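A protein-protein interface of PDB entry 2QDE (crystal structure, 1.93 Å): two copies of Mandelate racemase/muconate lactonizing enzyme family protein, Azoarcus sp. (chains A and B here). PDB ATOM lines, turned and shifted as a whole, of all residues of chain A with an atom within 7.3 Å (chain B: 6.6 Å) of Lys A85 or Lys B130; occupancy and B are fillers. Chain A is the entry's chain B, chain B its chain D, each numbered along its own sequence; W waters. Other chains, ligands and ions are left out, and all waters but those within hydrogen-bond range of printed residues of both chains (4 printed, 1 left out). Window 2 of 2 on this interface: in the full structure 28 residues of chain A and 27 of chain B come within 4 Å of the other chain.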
ATOM      1  N   VAL A  77      22.099 -17.777  41.371  1.00  0.00           N
ATOM      2  CA  VAL A  77      22.421 -17.004  40.174  1.00  0.00           C
ATOM      3  C   VAL A  77      23.788 -17.222  39.534  1.00  0.00           C
ATOM      4  O   VAL A  77      23.896 -17.316  38.312  1.00  0.00           O
ATOM      5  CB  VAL A  77      22.286 -15.482  40.468  1.00  0.00           C
ATOM      6  CG1 VAL A  77      22.631 -14.666  39.229  1.00  0.00           C
ATOM      7  CG2 VAL A  77      20.878 -15.169  40.943  1.00  0.00           C
ATOM      8  N   GLU A  81      26.685 -20.511  35.795  1.00  0.00           N
ATOM      9  CA  GLU A  81      26.393 -19.467  34.822  1.00  0.00           C
ATOM     10  C   GLU A  81      27.616 -18.970  34.046  1.00  0.00           C
ATOM     11  O   GLU A  81      28.750 -19.085  34.510  1.00  0.00           O
ATOM     12  CB  GLU A  81      25.728 -18.279  35.535  1.00  0.00           C
ATOM     13  CG  GLU A  81      25.377 -17.123  34.613  1.00  0.00           C
ATOM     14  CD  GLU A  81      24.315 -17.495  33.589  1.00  0.00           C
ATOM     15  OE1 GLU A  81      23.110 -17.384  33.905  1.00  0.00           O
ATOM     16  OE2 GLU A  81      24.686 -17.914  32.468  1.00  0.00           O
ATOM     17  N   ASP A  82      27.355 -18.415  32.863  1.00  0.00           N
ATOM     18  CA  ASP A  82      28.380 -17.844  31.996  1.00  0.00           C
ATOM     19  C   ASP A  82      28.646 -16.430  32.545  1.00  0.00           C
ATOM     20  O   ASP A  82      27.759 -15.578  32.550  1.00  0.00           O
ATOM     21  CB  ASP A  82      27.839 -17.764  30.562  1.00  0.00           C
ATOM     22  CG  ASP A  82      28.866 -17.278  29.559  1.00  0.00           C
ATOM     23  OD1 ASP A  82      29.789 -16.528  29.932  1.00  0.00           O
ATOM     24  OD2 ASP A  82      28.731 -17.637  28.369  1.00  0.00           O
ATOM     25  N   PRO A  83      29.879 -16.167  33.010  1.00  0.00           N
ATOM     26  CA  PRO A  83      30.248 -14.862  33.564  1.00  0.00           C
ATOM     27  C   PRO A  83      30.121 -13.665  32.621  1.00  0.00           C
ATOM     28  O   PRO A  83      30.115 -12.520  33.074  1.00  0.00           O
ATOM     29  CB  PRO A  83      31.688 -15.086  34.030  1.00  0.00           C
ATOM     30  CG  PRO A  83      32.212 -16.040  33.018  1.00  0.00           C
ATOM     31  CD  PRO A  83      31.066 -17.034  32.886  1.00  0.00           C
ATOM     32  N   THR A  84      30.017 -13.920  31.320  1.00  0.00           N
ATOM     33  CA  THR A  84      29.890 -12.827  30.359  1.00  0.00           C
ATOM     34  C   THR A  84      28.476 -12.243  30.365  1.00  0.00           C
ATOM     35  O   THR A  84      28.256 -11.135  29.881  1.00  0.00           O
ATOM     36  CB  THR A  84      30.198 -13.290  28.920  1.00  0.00           C
ATOM     37  OG1 THR A  84      29.311 -14.359  28.565  1.00  0.00           O
ATOM     38  CG2 THR A  84      31.649 -13.755  28.797  1.00  0.00           C
ATOM     39  N   LYS A  85      27.521 -12.998  30.900  1.00  0.00           N
ATOM     40  CA  LYS A  85      26.130 -12.541  30.953  1.00  0.00           C
ATOM     41  C   LYS A  85      25.900 -11.610  32.138  1.00  0.00           C
ATOM     42  O   LYS A  85      25.112 -11.902  33.045  1.00  0.00           O
ATOM     43  CB  LYS A  85      25.191 -13.743  31.021  1.00  0.00           C
ATOM     44  CG  LYS A  85      25.287 -14.607  29.783  1.00  0.00           C
ATOM     45  CD  LYS A  85      24.279 -15.732  29.776  1.00  0.00           C
ATOM     46  CE  LYS A  85      24.410 -16.524  28.489  1.00  0.00           C
ATOM     47  NZ  LYS A  85      23.355 -17.555  28.387  1.00  0.00           N
ATOM     48  N   ILE A  86      26.591 -10.478  32.104  1.00  0.00           N
ATOM     49  CA  ILE A  86      26.515  -9.482  33.163  1.00  0.00           C
ATOM     50  C   ILE A  86      25.147  -8.800  33.302  1.00  0.00           C
ATOM     51  O   ILE A  86      24.645  -8.658  34.416  1.00  0.00           O
ATOM     52  CB  ILE A  86      27.624  -8.423  32.980  1.00  0.00           C
ATOM     53  CG1 ILE A  86      28.993  -9.112  33.068  1.00  0.00           C
ATOM     54  CG2 ILE A  86      27.527  -7.358  34.062  1.00  0.00           C
ATOM     55  CD1 ILE A  86      30.164  -8.197  32.822  1.00  0.00           C
ATOM     56  N   GLU A  87      24.548  -8.373  32.192  1.00  0.00           N
ATOM     57  CA  GLU A  87      23.230  -7.737  32.262  1.00  0.00           C
ATOM     58  C   GLU A  87      22.244  -8.706  32.914  1.00  0.00           C
ATOM     59  O   GLU A  87      21.416  -8.313  33.736  1.00  0.00           O
ATOM     60  CB  GLU A  87      22.726  -7.369  30.860  1.00  0.00           C
ATOM     61  CG  GLU A  87      23.316  -6.095  30.264  1.00  0.00           C
ATOM     62  CD  GLU A  87      22.411  -4.880  30.432  1.00  0.00           C
ATOM     63  OE1 GLU A  87      21.249  -5.045  30.848  1.00  0.00           O
ATOM     64  OE2 GLU A  87      22.863  -3.758  30.126  1.00  0.00           O
ATOM     65  N   LYS A  88      22.346  -9.981  32.553  1.00  0.00           N
ATOM     66  CA  LYS A  88      21.454 -11.004  33.092  1.00  0.00           C
ATOM     67  C   LYS A  88      21.649 -11.232  34.584  1.00  0.00           C
ATOM     68  O   LYS A  88      20.693 -11.194  35.359  1.00  0.00           O
ATOM     69  CB  LYS A  88      21.662 -12.329  32.344  1.00  0.00           C
ATOM     70  CG  LYS A  88      20.782 -13.478  32.833  1.00  0.00           C
ATOM     71  CD  LYS A  88      21.162 -14.789  32.144  1.00  0.00           C
ATOM     72  CE  LYS A  88      20.251 -15.921  32.561  1.00  0.00           C
ATOM     73  NZ  LYS A  88      20.716 -17.232  32.021  1.00  0.00           N
ATOM     74  N   ILE A  89      22.890 -11.487  34.982  1.00  0.00           N
ATOM     75  CA  ILE A  89      23.205 -11.737  36.382  1.00  0.00           C
ATOM     76  C   ILE A  89      22.806 -10.548  37.262  1.00  0.00           C
ATOM     77  O   ILE A  89      22.155 -10.718  38.295  1.00  0.00           O
ATOM     78  CB  ILE A  89      24.717 -12.034  36.562  1.00  0.00           C
ATOM     79  CG1 ILE A  89      25.079 -13.328  35.819  1.00  0.00           C
ATOM     80  CG2 ILE A  89      25.053 -12.163  38.045  1.00  0.00           C
ATOM     81  CD1 ILE A  89      26.563 -13.611  35.759  1.00  0.00           C
ATOM     82  N   VAL A  90      23.203  -9.349  36.848  1.00  0.00           N
ATOM     83  CA  VAL A  90      22.867  -8.143  37.592  1.00  0.00           C
ATOM     84  C   VAL A  90      21.355  -8.058  37.758  1.00  0.00           C
ATOM     85  O   VAL A  90      20.864  -7.724  38.831  1.00  0.00           O
ATOM     86  CB  VAL A  90      23.383  -6.879  36.864  1.00  0.00           C
ATOM     87  CG1 VAL A  90      22.787  -5.619  37.491  1.00  0.00           C
ATOM     88  CG2 VAL A  90      24.898  -6.826  36.947  1.00  0.00           C
ATOM     89  N   GLY A  91      20.623  -8.371  36.691  1.00  0.00           N
ATOM     90  CA  GLY A  91      19.174  -8.325  36.748  1.00  0.00           C
ATOM     91  C   GLY A  91      18.614  -9.333  37.727  1.00  0.00           C
ATOM     92  O   GLY A  91      17.735  -9.016  38.531  1.00  0.00           O
ATOM     93  N   LEU A 111      32.865 -10.129  38.190  1.00  0.00           N
ATOM     94  CA  LEU A 111      32.404 -10.575  36.883  1.00  0.00           C
ATOM     95  C   LEU A 111      33.119  -9.794  35.785  1.00  0.00           C
ATOM     96  O   LEU A 111      33.527 -10.366  34.773  1.00  0.00           O
ATOM     97  CB  LEU A 111      30.893 -10.384  36.749  1.00  0.00           C
ATOM     98  CG  LEU A 111      30.037 -11.389  37.519  1.00  0.00           C
ATOM     99  CD1 LEU A 111      28.592 -10.926  37.542  1.00  0.00           C
ATOM    100  CD2 LEU A 111      30.165 -12.770  36.879  1.00  0.00           C
ATOM    101  N   VAL A 115      35.514 -11.420  32.949  1.00  0.00           N
ATOM    102  CA  VAL A 115      35.223 -11.223  31.527  1.00  0.00           C
ATOM    103  C   VAL A 115      36.409 -10.565  30.816  1.00  0.00           C
ATOM    104  O   VAL A 115      36.757 -10.938  29.690  1.00  0.00           O
ATOM    105  CB  VAL A 115      33.956 -10.348  31.326  1.00  0.00           C
ATOM    106  CG1 VAL A 115      33.777 -10.008  29.844  1.00  0.00           C
ATOM    107  CG2 VAL A 115      32.736 -11.087  31.841  1.00  0.00           C
ATOM    108  N   TYR B 124      26.918  -8.631  21.128  1.00  0.00           N
ATOM    109  CA  TYR B 124      26.119  -8.794  22.335  1.00  0.00           C
ATOM    110  C   TYR B 124      26.984  -8.960  23.584  1.00  0.00           C
ATOM    111  O   TYR B 124      26.541  -8.654  24.693  1.00  0.00           O
ATOM    112  CB  TYR B 124      25.109  -9.951  22.201  1.00  0.00           C
ATOM    113  CG  TYR B 124      25.661 -11.314  21.850  1.00  0.00           C
ATOM    114  CD1 TYR B 124      26.523 -11.994  22.712  1.00  0.00           C
ATOM    115  CD2 TYR B 124      25.274 -11.950  20.669  1.00  0.00           C
ATOM    116  CE1 TYR B 124      26.983 -13.286  22.404  1.00  0.00           C
ATOM    117  CE2 TYR B 124      25.723 -13.231  20.351  1.00  0.00           C
ATOM    118  CZ  TYR B 124      26.572 -13.897  21.221  1.00  0.00           C
ATOM    119  OH  TYR B 124      26.981 -15.183  20.911  1.00  0.00           O
ATOM    120  N   GLN B 125      28.217  -9.424  23.396  1.00  0.00           N
ATOM    121  CA  GLN B 125      29.156  -9.594  24.501  1.00  0.00           C
ATOM    122  C   GLN B 125      29.621  -8.217  24.979  1.00  0.00           C
ATOM    123  O   GLN B 125      29.996  -8.046  26.140  1.00  0.00           O
ATOM    124  CB  GLN B 125      30.375 -10.411  24.053  1.00  0.00           C
ATOM    125  CG  GLN B 125      30.048 -11.816  23.573  1.00  0.00           C
ATOM    126  CD  GLN B 125      29.577 -12.740  24.689  1.00  0.00           C
ATOM    127  OE1 GLN B 125      28.635 -12.423  25.426  1.00  0.00           O
ATOM    128  NE2 GLN B 125      30.224 -13.898  24.811  1.00  0.00           N
ATOM    129  N   GLY B 128      26.717  -6.439  27.289  1.00  0.00           N
ATOM    130  CA  GLY B 128      26.254  -7.087  28.506  1.00  0.00           C
ATOM    131  C   GLY B 128      26.035  -8.591  28.485  1.00  0.00           C
ATOM    132  O   GLY B 128      25.512  -9.154  29.453  1.00  0.00           O
ATOM    133  N   GLY B 129      26.422  -9.249  27.397  1.00  0.00           N
ATOM    134  CA  GLY B 129      26.254 -10.689  27.314  1.00  0.00           C
ATOM    135  C   GLY B 129      24.919 -11.107  26.729  1.00  0.00           C
ATOM    136  O   GLY B 129      24.004 -10.288  26.600  1.00  0.00           O
ATOM    137  N   LYS B 130      24.799 -12.386  26.385  1.00  0.00           N
ATOM    138  CA  LYS B 130      23.571 -12.905  25.794  1.00  0.00           C
ATOM    139  C   LYS B 130      22.549 -13.278  26.861  1.00  0.00           C
ATOM    140  O   LYS B 130      22.541 -14.409  27.357  1.00  0.00           O
ATOM    141  CB  LYS B 130      23.882 -14.126  24.917  1.00  0.00           C
ATOM    142  CG  LYS B 130      22.666 -14.662  24.171  1.00  0.00           C
ATOM    143  CD  LYS B 130      22.951 -15.958  23.421  1.00  0.00           C
ATOM    144  CE  LYS B 130      23.959 -15.770  22.312  1.00  0.00           C
ATOM    145  NZ  LYS B 130      24.049 -17.005  21.468  1.00  0.00           N
ATOM    146  N   THR B 131      21.682 -12.328  27.208  1.00  0.00           N
ATOM    147  CA  THR B 131      20.667 -12.554  28.229  1.00  0.00           C
ATOM    148  C   THR B 131      19.603 -13.551  27.775  1.00  0.00           C
ATOM    149  O   THR B 131      19.125 -14.358  28.568  1.00  0.00           O
ATOM    150  CB  THR B 131      20.008 -11.228  28.643  1.00  0.00           C
ATOM    151  OG1 THR B 131      21.028 -10.294  29.022  1.00  0.00           O
ATOM    152  CG2 THR B 131      19.069 -11.447  29.817  1.00  0.00           C
ATOM    153  N   ILE B 132      19.216 -13.486  26.507  1.00  0.00           N
ATOM    154  CA  ILE B 132      18.258 -14.443  25.968  1.00  0.00           C
ATOM    155  C   ILE B 132      18.857 -15.036  24.697  1.00  0.00           C
ATOM    156  O   ILE B 132      19.627 -14.373  24.000  1.00  0.00           O
ATOM    157  CB  ILE B 132      16.881 -13.805  25.660  1.00  0.00           C
ATOM    158  CG1 ILE B 132      17.043 -12.551  24.794  1.00  0.00           C
ATOM    159  CG2 ILE B 132      16.167 -13.494  26.963  1.00  0.00           C
ATOM    160  CD1 ILE B 132      15.709 -11.940  24.353  1.00  0.00           C
ATOM    161  N   GLU B 133      18.507 -16.282  24.401  1.00  0.00           N
ATOM    162  CA  GLU B 133      19.054 -16.968  23.233  1.00  0.00           C
ATOM    163  C   GLU B 133      18.373 -16.596  21.937  1.00  0.00           C
ATOM    164  O   GLU B 133      19.015 -16.548  20.889  1.00  0.00           O
ATOM    165  CB  GLU B 133      18.988 -18.482  23.430  1.00  0.00           C
ATOM    166  CG  GLU B 133      19.403 -18.928  24.820  1.00  0.00           C
ATOM    167  CD  GLU B 133      19.882 -20.376  24.867  1.00  0.00           C
ATOM    168  OE1 GLU B 133      19.207 -21.273  24.287  1.00  0.00           O
ATOM    169  OE2 GLU B 133      20.939 -20.616  25.499  1.00  0.00           O
ATOM    170  N   ARG B 134      17.069 -16.342  22.005  1.00  0.00           N
ATOM    171  CA  ARG B 134      16.305 -15.956  20.826  1.00  0.00           C
ATOM    172  C   ARG B 134      15.273 -14.899  21.208  1.00  0.00           C
ATOM    173  O   ARG B 134      14.799 -14.855  22.345  1.00  0.00           O
ATOM    174  CB  ARG B 134      15.618 -17.170  20.201  1.00  0.00           C
ATOM    175  CG  ARG B 134      14.616 -17.858  21.103  1.00  0.00           C
ATOM    176  CD  ARG B 134      14.049 -19.098  20.422  1.00  0.00           C
ATOM    177  NE  ARG B 134      13.016 -19.741  21.228  1.00  0.00           N
ATOM    178  CZ  ARG B 134      12.358 -20.832  20.851  1.00  0.00           C
ATOM    179  NH1 ARG B 134      12.631 -21.400  19.679  1.00  0.00           N
ATOM    180  NH2 ARG B 134      11.424 -21.354  21.636  1.00  0.00           N
ATOM    181  N   ALA B 314      19.040  -9.116  22.396  1.00  0.00           N
ATOM    182  CA  ALA B 314      19.418 -10.357  23.065  1.00  0.00           C
ATOM    183  C   ALA B 314      20.208 -10.072  24.346  1.00  0.00           C
ATOM    184  O   ALA B 314      20.199 -10.870  25.285  1.00  0.00           O
ATOM    185  CB  ALA B 314      20.265 -11.229  22.116  1.00  0.00           C
ATOM    186  N   ALA B 315      20.867  -8.919  24.387  1.00  0.00           N
ATOM    187  CA  ALA B 315      21.698  -8.553  25.528  1.00  0.00           C
ATOM    188  C   ALA B 315      21.064  -7.689  26.612  1.00  0.00           C
ATOM    189  O   ALA B 315      21.187  -7.997  27.794  1.00  0.00           O
ATOM    190  CB  ALA B 315      22.974  -7.879  25.029  1.00  0.00           C
ATOM    191  N   PRO B 359      20.398 -13.881  17.166  1.00  0.00           N
ATOM    192  CA  PRO B 359      21.550 -13.056  16.790  1.00  0.00           C
ATOM    193  C   PRO B 359      22.692 -13.940  16.269  1.00  0.00           C
ATOM    194  O   PRO B 359      22.859 -15.069  16.728  1.00  0.00           O
ATOM    195  CB  PRO B 359      21.912 -12.360  18.100  1.00  0.00           C
ATOM    196  CG  PRO B 359      21.548 -13.408  19.135  1.00  0.00           C
ATOM    197  CD  PRO B 359      20.213 -13.907  18.630  1.00  0.00           C
ATOM    198  N   ASN B 360      23.453 -13.441  15.295  1.00  0.00           N
ATOM    199  CA  ASN B 360      24.584 -14.200  14.756  1.00  0.00           C
ATOM    200  C   ASN B 360      25.625 -14.291  15.873  1.00  0.00           C
ATOM    201  O   ASN B 360      25.666 -13.425  16.754  1.00  0.00           O
ATOM    202  CB  ASN B 360      25.185 -13.496  13.536  1.00  0.00           C
ATOM    203  CG  ASN B 360      24.454 -13.834  12.239  1.00  0.00           C
ATOM    204  OD1 ASN B 360      24.766 -13.284  11.175  1.00  0.00           O
ATOM    205  ND2 ASN B 360      23.486 -14.745  12.319  1.00  0.00           N
ATOM    206  N   ASP B 361      26.464 -15.324  15.836  1.00  0.00           N
ATOM    207  CA  ASP B 361      27.470 -15.519  16.877  1.00  0.00           C
ATOM    208  C   ASP B 361      28.917 -15.229  16.479  1.00  0.00           C
ATOM    209  O   ASP B 361      29.837 -15.489  17.258  1.00  0.00           O
ATOM    210  CB  ASP B 361      27.372 -16.948  17.426  1.00  0.00           C
ATOM    211  CG  ASP B 361      26.056 -17.205  18.158  1.00  0.00           C
ATOM    212  OD1 ASP B 361      25.770 -16.483  19.143  1.00  0.00           O
ATOM    213  OD2 ASP B 361      25.307 -18.122  17.759  1.00  0.00           O
HETATM  214  O   HOH W   1      27.122 -14.020  26.764  1.00  0.00           O
HETATM  215  O   HOH W   2      29.812 -16.663  26.245  1.00  0.00           O
HETATM  216  O   HOH W   3      20.272 -17.058  29.283  1.00  0.00           O
HETATM  217  O   HOH W   4      29.972  -9.111  28.785  1.00  0.00           O
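The side-chain carboxylate (OE1) of Glu A81 is in salt-bridge range of the side-chain amino group (NZ) of Lys A88.
The backbone carbonyl oxygen (O) of Tyr B124 is in hydrogen-bond range of the backbone NH (N) of Gly B129 (2.8 Å).
The side-chain hydroxyl (OH) of Tyr B124 sits close to the side-chain amino group (NZ) of Lys B130, at 3.5 Å.
OD1 of Asp B361 lies within salt-bridge range of NZ of Lys B130, at 2.9 Å.
N of Thr B131 lies within hydrogen-bond range of O of Ala B314, at 2.8 Å.
OG1 of Thr B131 sits at hydrogen-bond distance from O of Ala B315 (2.6 Å).
No position is printed for both chains.
Of the 10 pairs that touch across the chains among the printed residues, none has its exchanged pair printed and touching as well.
Water W2 lies within hydrogen-bond range of OD2 of Asp A82, NE2 of Gln B125 and OG1 of Thr A84.
Water W1 lies within hydrogen-bond range of the side-chain amide oxygen of Gln B125 (2.6 Å), the side-chain hydroxyl of Thr A84 (2.9 Å) and the backbone NH of Lys B130 (2.9 Å).
Water W3 lies within hydrogen-bond range of the side-chain amino group (NZ) of Lys A88 (2.8 Å), the backbone carbonyl oxygen (O) of Thr B131 (3.0 Å) and the side-chain amino group (NZ) of Lys A85 (3.2 Å).
Water W4 lies within hydrogen-bond range of O of Gln B125 (2.9 Å) and O of Thr A84 (2.9 Å).
Printed residues of chain A that touch a printed residue of chain B: Thr A84, Lys A85, Ile A86, Glu A87 and Lys A88.
Of the 14 printed residues of chain B, 6 touch a printed residue of chain A.
Printed residues of chain B that touch a printed residue of chain A: Gln B125, Gly B128, Gly B129, Lys B130, Thr B131 and Ala B315.
Along chain B the printed residues that touch a printed residue of chain A span positions 125 to 315.
Among the printed residues, 10 pairs touch across the chains.
Among the printed residues, pairs that only touch across the chains: Thr A84 with Gln B125 (3.7 Å), Thr A84 with Gly B129 (3.3 Å), Lys A85 with Gly B128 (3.7 Å), Glu A87 with Thr B131 (3.8 Å), Glu A87 with Ala B315 (3.5 Å) and Lys A88 with Thr B131 (3.7 Å).
O of Lys B130 lies close to NZ of Lys A85.
The backbone NH (N) of Ile A86 lies within hydrogen-bond range of the backbone carbonyl oxygen (O) of Gly B128 (3.2 Å).
The backbone carbonyl oxygen (O) of Gly B128 is in hydrogen-bond range of the backbone NH (N) of Glu A87, at 3.0 Å.
The backbone carbonyl oxygen (O) of Gly B128 sits close to the backbone carbonyl oxygen (O) of Thr A84.
Of chain B, only Gly B128 (3.7 Å) and Lys B130 (3.0 Å) come within 4 Å of Lys A85.
Lys B130 touches one residue of chain A.
Printed residues of chain A within 4 Å of Gly B128: Thr A84 (3.4 Å), Lys A85 (3.7 Å), Ile A86 (3.2 Å) and Glu A87 (3.0 Å).
Printed residues of chain A within 4 Å of Ala B315: Glu A87.
Of the printed residues of chain B, Ile A86 touches Gly B128.
Of the printed residues of chain A, Thr B131 touches Glu A87 (3.8 Å) and Lys A88 (3.7 Å).
The nearest residue of chain A that does not touch Lys B130 is Lys A88 (5.0 Å).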
